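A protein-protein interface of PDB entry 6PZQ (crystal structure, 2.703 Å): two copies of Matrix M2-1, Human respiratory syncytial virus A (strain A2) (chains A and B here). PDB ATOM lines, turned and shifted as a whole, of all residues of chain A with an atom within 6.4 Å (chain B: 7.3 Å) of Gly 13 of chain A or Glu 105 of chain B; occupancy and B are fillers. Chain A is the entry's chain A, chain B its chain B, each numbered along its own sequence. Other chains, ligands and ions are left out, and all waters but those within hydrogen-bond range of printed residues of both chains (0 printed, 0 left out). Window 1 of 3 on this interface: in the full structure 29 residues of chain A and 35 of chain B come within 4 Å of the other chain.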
ATOM      1  N   LYS A   8      13.379   5.117   4.597  1.00  0.00           N
ATOM      2  CA  LYS A   8      14.251   4.349   3.686  1.00  0.00           C
ATOM      3  C   LYS A   8      15.401   3.630   4.401  1.00  0.00           C
ATOM      4  O   LYS A   8      15.954   2.671   3.856  1.00  0.00           O
ATOM      5  CB  LYS A   8      14.830   5.254   2.600  1.00  0.00           C
ATOM      6  CG  LYS A   8      13.859   5.529   1.428  1.00  0.00           C
ATOM      7  CD  LYS A   8      14.490   6.352   0.279  1.00  0.00           C
ATOM      8  CE  LYS A   8      13.473   7.265  -0.408  1.00  0.00           C
ATOM      9  NZ  LYS A   8      14.048   8.646  -0.632  1.00  0.00           N
ATOM     10  N   PHE A   9      15.789   4.048   5.597  1.00  0.00           N
ATOM     11  CA  PHE A   9      16.708   3.209   6.341  1.00  0.00           C
ATOM     12  C   PHE A   9      16.032   1.908   6.738  1.00  0.00           C
ATOM     13  O   PHE A   9      16.619   0.834   6.596  1.00  0.00           O
ATOM     14  CB  PHE A   9      17.243   3.957   7.563  1.00  0.00           C
ATOM     15  CG  PHE A   9      18.200   5.038   7.200  1.00  0.00           C
ATOM     16  CD1 PHE A   9      19.545   4.728   6.968  1.00  0.00           C
ATOM     17  CD2 PHE A   9      17.772   6.353   7.029  1.00  0.00           C
ATOM     18  CE1 PHE A   9      20.466   5.715   6.582  1.00  0.00           C
ATOM     19  CE2 PHE A   9      18.676   7.353   6.634  1.00  0.00           C
ATOM     20  CZ  PHE A   9      20.023   7.038   6.415  1.00  0.00           C
ATOM     21  N   GLU A  10      14.796   1.979   7.235  1.00  0.00           N
ATOM     22  CA  GLU A  10      14.086   0.773   7.651  1.00  0.00           C
ATOM     23  C   GLU A  10      13.768  -0.110   6.455  1.00  0.00           C
ATOM     24  O   GLU A  10      13.759  -1.343   6.571  1.00  0.00           O
ATOM     25  CB  GLU A  10      12.810   1.165   8.378  1.00  0.00           C
ATOM     26  CG  GLU A  10      11.982   0.035   8.965  1.00  0.00           C
ATOM     27  CD  GLU A  10      12.478  -0.512  10.305  1.00  0.00           C
ATOM     28  OE1 GLU A  10      13.238   0.190  11.013  1.00  0.00           O
ATOM     29  OE2 GLU A  10      12.092  -1.675  10.638  1.00  0.00           O
ATOM     30  N   ILE A  11      13.532   0.496   5.291  1.00  0.00           N
ATOM     31  CA  ILE A  11      13.335  -0.295   4.079  1.00  0.00           C
ATOM     32  C   ILE A  11      14.498  -1.233   3.812  1.00  0.00           C
ATOM     33  O   ILE A  11      14.309  -2.320   3.260  1.00  0.00           O
ATOM     34  CB  ILE A  11      13.126   0.596   2.872  1.00  0.00           C
ATOM     35  CG1 ILE A  11      11.793   1.338   3.024  1.00  0.00           C
ATOM     36  CG2 ILE A  11      13.205  -0.275   1.633  1.00  0.00           C
ATOM     37  CD1 ILE A  11      11.352   2.150   1.834  1.00  0.00           C
ATOM     38  N   ARG A  12      15.706  -0.834   4.162  1.00  0.00           N
ATOM     39  CA  ARG A  12      16.888  -1.662   3.990  1.00  0.00           C
ATOM     40  C   ARG A  12      17.250  -2.478   5.234  1.00  0.00           C
ATOM     41  O   ARG A  12      18.365  -3.013   5.307  1.00  0.00           O
ATOM     42  CB  ARG A  12      18.070  -0.789   3.579  1.00  0.00           C
ATOM     43  CG  ARG A  12      17.860  -0.218   2.231  1.00  0.00           C
ATOM     44  CD  ARG A  12      19.028   0.711   1.850  1.00  0.00           C
ATOM     45  NE  ARG A  12      18.864   1.149   0.460  1.00  0.00           N
ATOM     46  CZ  ARG A  12      19.509   0.631  -0.577  1.00  0.00           C
ATOM     47  NH1 ARG A  12      20.424  -0.332  -0.416  1.00  0.00           N
ATOM     48  NH2 ARG A  12      19.239   1.099  -1.786  1.00  0.00           N
ATOM     49  N   GLY A  13      16.347  -2.585   6.206  1.00  0.00           N
ATOM     50  CA  GLY A  13      16.632  -3.348   7.400  1.00  0.00           C
ATOM     51  C   GLY A  13      16.055  -2.688   8.630  1.00  0.00           C
ATOM     52  O   GLY A  13      14.841  -2.750   8.863  1.00  0.00           O
ATOM     53  N   HIS A  14      16.939  -2.071   9.425  1.00  0.00           N
ATOM     54  CA  HIS A  14      16.598  -1.424  10.691  1.00  0.00           C
ATOM     55  C   HIS A  14      17.138   0.011  10.722  1.00  0.00           C
ATOM     56  O   HIS A  14      18.329   0.221  10.452  1.00  0.00           O
ATOM     57  CB  HIS A  14      17.162  -2.224  11.859  1.00  0.00           C
ATOM     58  CG  HIS A  14      16.650  -1.764  13.194  1.00  0.00           C
ATOM     59  ND1 HIS A  14      15.306  -1.605  13.460  1.00  0.00           N
ATOM     60  CD2 HIS A  14      17.296  -1.434  14.336  1.00  0.00           C
ATOM     61  CE1 HIS A  14      15.147  -1.193  14.707  1.00  0.00           C
ATOM     62  NE2 HIS A  14      16.340  -1.082  15.260  1.00  0.00           N
ATOM     63  N   CYS A  15      16.276   0.991  11.052  1.00  0.00           N
ATOM     64  CA  CYS A  15      16.719   2.380  11.205  1.00  0.00           C
ATOM     65  C   CYS A  15      17.536   2.518  12.462  1.00  0.00           C
ATOM     66  O   CYS A  15      17.151   1.998  13.503  1.00  0.00           O
ATOM     67  CB  CYS A  15      15.556   3.362  11.306  1.00  0.00           C
ATOM     68  SG  CYS A  15      15.987   5.109  11.584  1.00  0.00           S
ATOM     69  N   LEU A  16      18.648   3.262  12.367  1.00  0.00           N
ATOM     70  CA  LEU A  16      19.563   3.439  13.482  1.00  0.00           C
ATOM     71  C   LEU A  16      19.584   4.868  14.021  1.00  0.00           C
ATOM     72  O   LEU A  16      20.429   5.176  14.872  1.00  0.00           O
ATOM     73  CB  LEU A  16      20.978   3.022  13.067  1.00  0.00           C
ATOM     74  CG  LEU A  16      21.215   1.516  12.895  1.00  0.00           C
ATOM     75  CD1 LEU A  16      22.614   1.226  12.438  1.00  0.00           C
ATOM     76  CD2 LEU A  16      20.918   0.780  14.151  1.00  0.00           C
ATOM     77  N   TYR A  27       4.858  -0.740   9.785  1.00  0.00           N
ATOM     78  CA  TYR A  27       4.516  -1.380   8.509  1.00  0.00           C
ATOM     79  C   TYR A  27       3.022  -1.254   8.154  1.00  0.00           C
ATOM     80  O   TYR A  27       2.658  -1.306   6.966  1.00  0.00           O
ATOM     81  CB  TYR A  27       4.923  -2.862   8.562  1.00  0.00           C
ATOM     82  CG  TYR A  27       6.331  -3.114   9.037  1.00  0.00           C
ATOM     83  CD1 TYR A  27       7.379  -2.379   8.540  1.00  0.00           C
ATOM     84  CD2 TYR A  27       6.614  -4.122   9.957  1.00  0.00           C
ATOM     85  CE1 TYR A  27       8.659  -2.594   8.986  1.00  0.00           C
ATOM     86  CE2 TYR A  27       7.906  -4.359  10.384  1.00  0.00           C
ATOM     87  CZ  TYR A  27       8.928  -3.592   9.876  1.00  0.00           C
ATOM     88  OH  TYR A  27      10.240  -3.768  10.227  1.00  0.00           O
ATOM     89  N   ARG A  38      11.438  -4.042   1.170  1.00  0.00           N
ATOM     90  CA  ARG A  38      11.989  -4.438   2.467  1.00  0.00           C
ATOM     91  C   ARG A  38      12.215  -5.936   2.532  1.00  0.00           C
ATOM     92  O   ARG A  38      13.325  -6.389   2.808  1.00  0.00           O
ATOM     93  CB  ARG A  38      11.084  -4.067   3.614  1.00  0.00           C
ATOM     94  CG  ARG A  38      11.881  -3.940   4.813  1.00  0.00           C
ATOM     95  CD  ARG A  38      11.129  -3.496   6.036  1.00  0.00           C
ATOM     96  NE  ARG A  38      12.024  -3.725   7.141  1.00  0.00           N
ATOM     97  CZ  ARG A  38      12.004  -4.817   7.896  1.00  0.00           C
ATOM     98  NH1 ARG A  38      11.106  -5.789   7.688  1.00  0.00           N
ATOM     99  NH2 ARG A  38      12.869  -4.925   8.888  1.00  0.00           N
ATOM    100  N   PHE A  41      15.201  -6.971   0.707  1.00  0.00           N
ATOM    101  CA  PHE A  41      16.482  -6.710   1.387  1.00  0.00           C
ATOM    102  C   PHE A  41      16.662  -7.641   2.599  1.00  0.00           C
ATOM    103  O   PHE A  41      17.781  -8.116   2.889  1.00  0.00           O
ATOM    104  CB  PHE A  41      16.580  -5.240   1.806  1.00  0.00           C
ATOM    105  CG  PHE A  41      16.878  -4.300   0.685  1.00  0.00           C
ATOM    106  CD1 PHE A  41      18.158  -4.234   0.147  1.00  0.00           C
ATOM    107  CD2 PHE A  41      15.906  -3.445   0.201  1.00  0.00           C
ATOM    108  CE1 PHE A  41      18.470  -3.361  -0.859  1.00  0.00           C
ATOM    109  CE2 PHE A  41      16.200  -2.595  -0.852  1.00  0.00           C
ATOM    110  CZ  PHE A  41      17.504  -2.537  -1.368  1.00  0.00           C
ATOM    111  N   MET A  42      15.554  -7.910   3.304  1.00  0.00           N
ATOM    112  CA  MET A  42      15.548  -8.735   4.509  1.00  0.00           C
ATOM    113  C   MET A  42      15.833 -10.201   4.185  1.00  0.00           C
ATOM    114  O   MET A  42      16.494 -10.891   4.975  1.00  0.00           O
ATOM    115  CB  MET A  42      14.189  -8.631   5.206  1.00  0.00           C
ATOM    116  CG  MET A  42      13.958  -7.411   6.058  1.00  0.00           C
ATOM    117  SD  MET A  42      15.276  -7.127   7.288  1.00  0.00           S
ATOM    118  CE  MET A  42      14.768  -8.285   8.578  1.00  0.00           C
ATOM    119  N   ARG A  45      19.438 -10.440   3.821  1.00  0.00           N
ATOM    120  CA  ARG A  45      20.261 -10.519   5.038  1.00  0.00           C
ATOM    121  C   ARG A  45      20.174 -11.916   5.624  1.00  0.00           C
ATOM    122  O   ARG A  45      21.176 -12.457   6.109  1.00  0.00           O
ATOM    123  CB  ARG A  45      19.902  -9.476   6.130  1.00  0.00           C
ATOM    124  CG  ARG A  45      20.077  -7.979   5.788  1.00  0.00           C
ATOM    125  CD  ARG A  45      19.890  -6.965   7.013  1.00  0.00           C
ATOM    126  NE  ARG A  45      20.695  -7.389   8.171  1.00  0.00           N
ATOM    127  CZ  ARG A  45      20.648  -6.876   9.415  1.00  0.00           C
ATOM    128  NH1 ARG A  45      19.804  -5.865   9.729  1.00  0.00           N
ATOM    129  NH2 ARG A  45      21.454  -7.399  10.369  1.00  0.00           N
ATOM    130  N   ASN B  40       6.742  -8.874   6.766  1.00  0.00           N
ATOM    131  CA  ASN B  40       7.825  -8.099   7.377  1.00  0.00           C
ATOM    132  C   ASN B  40       7.938  -8.351   8.902  1.00  0.00           C
ATOM    133  O   ASN B  40       9.060  -8.464   9.435  1.00  0.00           O
ATOM    134  CB  ASN B  40       7.620  -6.628   7.062  1.00  0.00           C
ATOM    135  CG  ASN B  40       8.144  -6.237   5.692  1.00  0.00           C
ATOM    136  OD1 ASN B  40       9.346  -6.066   5.484  1.00  0.00           O
ATOM    137  ND2 ASN B  40       7.245  -6.079   4.754  1.00  0.00           N
ATOM    138  N   ASN B  44      11.453 -10.110  10.393  1.00  0.00           N
ATOM    139  CA  ASN B  44      12.200  -9.524  11.492  1.00  0.00           C
ATOM    140  C   ASN B  44      12.441 -10.573  12.551  1.00  0.00           C
ATOM    141  O   ASN B  44      13.444 -10.529  13.278  1.00  0.00           O
ATOM    142  CB  ASN B  44      11.452  -8.296  12.057  1.00  0.00           C
ATOM    143  CG  ASN B  44      11.473  -7.074  11.074  1.00  0.00           C
ATOM    144  OD1 ASN B  44      12.070  -7.113   9.987  1.00  0.00           O
ATOM    145  ND2 ASN B  44      10.795  -6.017  11.452  1.00  0.00           N
ATOM    146  N   LEU B  47      15.166 -13.312  11.408  1.00  0.00           N
ATOM    147  CA  LEU B  47      16.495 -12.720  11.486  1.00  0.00           C
ATOM    148  C   LEU B  47      16.988 -12.609  12.912  1.00  0.00           C
ATOM    149  O   LEU B  47      18.155 -12.884  13.192  1.00  0.00           O
ATOM    150  CB  LEU B  47      16.497 -11.343  10.878  1.00  0.00           C
ATOM    151  CG  LEU B  47      17.879 -10.670  10.773  1.00  0.00           C
ATOM    152  CD1 LEU B  47      18.973 -11.580  10.152  1.00  0.00           C
ATOM    153  CD2 LEU B  47      17.710  -9.434   9.913  1.00  0.00           C
ATOM    154  N   MET B  99      29.371   1.162  17.142  1.00  0.00           N
ATOM    155  CA  MET B  99      30.014   1.018  15.835  1.00  0.00           C
ATOM    156  C   MET B  99      29.830  -0.388  15.284  1.00  0.00           C
ATOM    157  O   MET B  99      29.647  -0.568  14.074  1.00  0.00           O
ATOM    158  CB  MET B  99      31.499   1.354  15.913  1.00  0.00           C
ATOM    159  CG  MET B  99      32.269   1.170  14.581  1.00  0.00           C
ATOM    160  SD  MET B  99      31.528   2.064  13.224  1.00  0.00           S
ATOM    161  CE  MET B  99      32.786   1.920  11.998  1.00  0.00           C
ATOM    162  N   SER B 100      29.850  -1.401  16.143  1.00  0.00           N
ATOM    163  CA  SER B 100      29.553  -2.734  15.628  1.00  0.00           C
ATOM    164  C   SER B 100      28.106  -2.861  15.163  1.00  0.00           C
ATOM    165  O   SER B 100      27.860  -3.440  14.106  1.00  0.00           O
ATOM    166  CB  SER B 100      29.840  -3.817  16.650  1.00  0.00           C
ATOM    167  OG  SER B 100      29.071  -4.921  16.255  1.00  0.00           O
ATOM    168  N   LYS B 101      27.135  -2.340  15.923  1.00  0.00           N
ATOM    169  CA  LYS B 101      25.748  -2.335  15.444  1.00  0.00           C
ATOM    170  C   LYS B 101      25.654  -1.787  14.034  1.00  0.00           C
ATOM    171  O   LYS B 101      24.831  -2.249  13.239  1.00  0.00           O
ATOM    172  CB  LYS B 101      24.817  -1.453  16.291  1.00  0.00           C
ATOM    173  CG  LYS B 101      24.627  -1.787  17.742  1.00  0.00           C
ATOM    174  CD  LYS B 101      23.477  -2.643  17.999  1.00  0.00           C
ATOM    175  CE  LYS B 101      23.169  -2.592  19.462  1.00  0.00           C
ATOM    176  NZ  LYS B 101      24.409  -2.491  20.258  1.00  0.00           N
ATOM    177  N   LEU B 102      26.431  -0.729  13.739  1.00  0.00           N
ATOM    178  CA  LEU B 102      26.303  -0.042  12.460  1.00  0.00           C
ATOM    179  C   LEU B 102      26.905  -0.888  11.381  1.00  0.00           C
ATOM    180  O   LEU B 102      26.363  -0.972  10.271  1.00  0.00           O
ATOM    181  CB  LEU B 102      26.983   1.323  12.478  1.00  0.00           C
ATOM    182  CG  LEU B 102      27.065   2.010  11.123  1.00  0.00           C
ATOM    183  CD1 LEU B 102      25.696   2.209  10.497  1.00  0.00           C
ATOM    184  CD2 LEU B 102      27.783   3.293  11.203  1.00  0.00           C
ATOM    185  N   LEU B 103      28.013  -1.547  11.713  1.00  0.00           N
ATOM    186  CA  LEU B 103      28.643  -2.446  10.764  1.00  0.00           C
ATOM    187  C   LEU B 103      27.684  -3.556  10.377  1.00  0.00           C
ATOM    188  O   LEU B 103      27.566  -3.895   9.187  1.00  0.00           O
ATOM    189  CB  LEU B 103      29.931  -3.019  11.361  1.00  0.00           C
ATOM    190  CG  LEU B 103      31.028  -1.992  11.540  1.00  0.00           C
ATOM    191  CD1 LEU B 103      32.149  -2.593  12.335  1.00  0.00           C
ATOM    192  CD2 LEU B 103      31.484  -1.478  10.174  1.00  0.00           C
ATOM    193  N   THR B 104      26.945  -4.110  11.365  1.00  0.00           N
ATOM    194  CA  THR B 104      26.177  -5.279  10.988  1.00  0.00           C
ATOM    195  C   THR B 104      24.966  -4.931  10.144  1.00  0.00           C
ATOM    196  O   THR B 104      24.303  -5.854   9.652  1.00  0.00           O
ATOM    197  CB  THR B 104      25.694  -6.108  12.170  1.00  0.00           C
ATOM    198  OG1 THR B 104      24.301  -5.901  12.301  1.00  0.00           O
ATOM    199  CG2 THR B 104      26.411  -5.856  13.472  1.00  0.00           C
ATOM    200  N   GLU B 105      24.692  -3.641   9.940  1.00  0.00           N
ATOM    201  CA  GLU B 105      23.552  -3.168   9.173  1.00  0.00           C
ATOM    202  C   GLU B 105      23.961  -2.712   7.792  1.00  0.00           C
ATOM    203  O   GLU B 105      23.120  -2.604   6.886  1.00  0.00           O
ATOM    204  CB  GLU B 105      22.868  -2.009   9.955  1.00  0.00           C
ATOM    205  CG  GLU B 105      21.679  -1.279   9.274  1.00  0.00           C
ATOM    206  CD  GLU B 105      20.391  -2.122   9.232  1.00  0.00           C
ATOM    207  OE1 GLU B 105      20.211  -2.973  10.151  1.00  0.00           O
ATOM    208  OE2 GLU B 105      19.570  -1.931   8.276  1.00  0.00           O
ATOM    209  N   LEU B 106      25.222  -2.388   7.614  1.00  0.00           N
ATOM    210  CA  LEU B 106      25.728  -2.229   6.263  1.00  0.00           C
ATOM    211  C   LEU B 106      25.860  -3.601   5.610  1.00  0.00           C
ATOM    212  O   LEU B 106      26.079  -4.618   6.286  1.00  0.00           O
ATOM    213  CB  LEU B 106      27.075  -1.496   6.292  1.00  0.00           C
ATOM    214  CG  LEU B 106      26.986  -0.093   6.870  1.00  0.00           C
ATOM    215  CD1 LEU B 106      28.405   0.394   7.110  1.00  0.00           C
ATOM    216  CD2 LEU B 106      26.173   0.838   5.917  1.00  0.00           C
ATOM    217  N   ASN B 107      25.705  -3.638   4.293  1.00  0.00           N
ATOM    218  CA  ASN B 107      25.988  -4.855   3.547  1.00  0.00           C
ATOM    219  C   ASN B 107      27.162  -4.567   2.611  1.00  0.00           C
ATOM    220  O   ASN B 107      27.101  -3.658   1.773  1.00  0.00           O
ATOM    221  CB  ASN B 107      24.714  -5.396   2.843  1.00  0.00           C
ATOM    222  CG  ASN B 107      24.582  -4.993   1.376  1.00  0.00           C
ATOM    223  OD1 ASN B 107      24.837  -5.805   0.485  1.00  0.00           O
ATOM    224  ND2 ASN B 107      24.125  -3.767   1.121  1.00  0.00           N
ATOM    225  N   SER B 108      28.243  -5.334   2.796  1.00  0.00           N
ATOM    226  CA  SER B 108      29.479  -5.139   2.048  1.00  0.00           C
ATOM    227  C   SER B 108      29.246  -5.069   0.549  1.00  0.00           C
ATOM    228  O   SER B 108      29.982  -4.371  -0.153  1.00  0.00           O
ATOM    229  CB  SER B 108      30.456  -6.261   2.385  1.00  0.00           C
ATOM    230  OG  SER B 108      29.752  -7.322   3.000  1.00  0.00           O
ATOM    231  N   ILE B 135      33.162  -4.425   8.430  1.00  0.00           N
ATOM    232  CA  ILE B 135      31.878  -5.118   8.388  1.00  0.00           C
ATOM    233  C   ILE B 135      32.100  -6.624   8.312  1.00  0.00           C
ATOM    234  O   ILE B 135      31.343  -7.404   8.917  1.00  0.00           O
ATOM    235  CB  ILE B 135      30.993  -4.592   7.222  1.00  0.00           C
ATOM    236  CG1 ILE B 135      29.821  -5.515   6.956  1.00  0.00           C
ATOM    237  CG2 ILE B 135      31.723  -4.509   5.936  1.00  0.00           C
ATOM    238  CD1 ILE B 135      28.958  -4.999   5.824  1.00  0.00           C
ATOM    239  N   ASN B 138      33.581  -7.877  11.620  1.00  0.00           N
ATOM    240  CA  ASN B 138      32.530  -7.814  12.618  1.00  0.00           C
ATOM    241  C   ASN B 138      31.527  -8.948  12.423  1.00  0.00           C
ATOM    242  O   ASN B 138      31.014  -9.495  13.409  1.00  0.00           O
ATOM    243  CB  ASN B 138      31.874  -6.426  12.569  1.00  0.00           C
ATOM    244  CG  ASN B 138      30.689  -6.275  13.537  1.00  0.00           C
ATOM    245  OD1 ASN B 138      29.564  -6.090  13.109  1.00  0.00           O
ATOM    246  ND2 ASN B 138      30.942  -6.362  14.830  1.00  0.00           N
ATOM    247  N   HIS B 168      26.994   4.757   4.985  1.00  0.00           N
ATOM    248  CA  HIS B 168      25.638   4.468   5.448  1.00  0.00           C
ATOM    249  C   HIS B 168      24.611   5.430   4.887  1.00  0.00           C
ATOM    250  O   HIS B 168      23.525   5.011   4.495  1.00  0.00           O
ATOM    251  CB  HIS B 168      25.606   4.513   6.977  1.00  0.00           C
ATOM    252  CG  HIS B 168      24.345   3.994   7.596  1.00  0.00           C
ATOM    253  ND1 HIS B 168      23.574   4.748   8.454  1.00  0.00           N
ATOM    254  CD2 HIS B 168      23.771   2.774   7.561  1.00  0.00           C
ATOM    255  CE1 HIS B 168      22.556   4.026   8.882  1.00  0.00           C
ATOM    256  NE2 HIS B 168      22.662   2.821   8.363  1.00  0.00           N
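No position is printed for both chains.
Of the 14 pairs that touch across the chains among the printed residues, none has its exchanged pair printed and touching as well.
Of chain B, only Glu 105 comes within 4 Å of Gly 13 of chain A.
Of chain A, only Arg 12, Gly 13, His 14 and Arg 45 come within 4 Å of Glu 105 of chain B.
Printed residues of chain B within 4 Å of Phe 9 of chain A: His 168.
Printed residues of chain B within 4 Å of Tyr 27 of chain A: Asn 40 and Asn 44.
Of the printed residues of chain A, Leu 102 of chain B touches Leu 16.
Met 99 of chain B touches none of the printed residues of chain A.
Ile 11 of chain A touches none of the printed residues of chain B.
OE2 of Glu 10 of chain A is in hydrogen-bond range of OH of Tyr 27 of chain A.
The side-chain carboxylate of Glu 10 of chain A lies within salt-bridge range of the guanidinium group of Arg 38 of chain A, at 3.8 Å.
The backbone carbonyl oxygen of Gly 13 of chain A is in hydrogen-bond range of the guanidinium group of Arg 38 of chain A (2.9 Å).
OH of Tyr 27 of chain A lies close to NH2 of Arg 38 of chain A (3.2 Å).
NH2 of Arg 38 of chain A lies within hydrogen-bond range of SD of Met 42 of chain A (3.6 Å).
The backbone carbonyl oxygen of Asn 40 of chain B sits close to the side-chain amide oxygen of Asn 44 of chain B (3.3 Å).
Hydrophobic or aromatic side chains of chain A within 4 Å of the printed part of chain B: Phe 9, His 14, Leu 16, Tyr 27 and Met 42.
Of the 16 printed residues of chain B, 7 touch a printed residue of chain A.
Among the printed residues, Asp or Glu carboxylates within 4 Å of a Lys or Arg side-chain nitrogen of the other chain: Arg 45 of chain A with Glu 105 of chain B.
N of His 14 of chain A sits at hydrogen-bond distance from OE2 of Glu 105 of chain B, at 2.9 Å.
OH of Tyr 27 of chain A is in hydrogen-bond range of ND2 of Asn 44 of chain B (2.6 Å).
OD1 of Asn 40 of chain B sits at hydrogen-bond distance from NH1 of Arg 38 of chain A.
NH2 of Arg 38 of chain A lies within hydrogen-bond range of OD1 of Asn 44 of chain B, 2.6 Å away.
The guanidinium group (NH2) of Arg 45 of chain A is in hydrogen-bond range of the backbone carbonyl oxygen (O) of Thr 104 of chain B.
The guanidinium group (NH1) of Arg 45 of chain A lies within salt-bridge range of the side-chain carboxylate (OE1) of Glu 105 of chain B (3.0 Å).
The side-chain carboxylate (OE2) of Glu 105 of chain B sits close to the backbone carbonyl oxygen (O) of Arg 12 of chain A.
Among the printed residues, merely in contact across the chains: Met 42 of chain A with Asn 44 of chain B (3.3 Å), Gly 13 of chain A with Glu 105 of chain B (3.4 Å), Met 42 of chain A with Leu 47 of chain B (3.4 Å), Phe 9 of chain A with His 168 of chain B (3.5 Å), Leu 16 of chain A with Leu 102 of chain B (3.8 Å), Arg 45 of chain A with Leu 47 of chain B (3.9 Å) and Tyr 27 of chain A with Asn 40 of chain B (3.96 Å).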
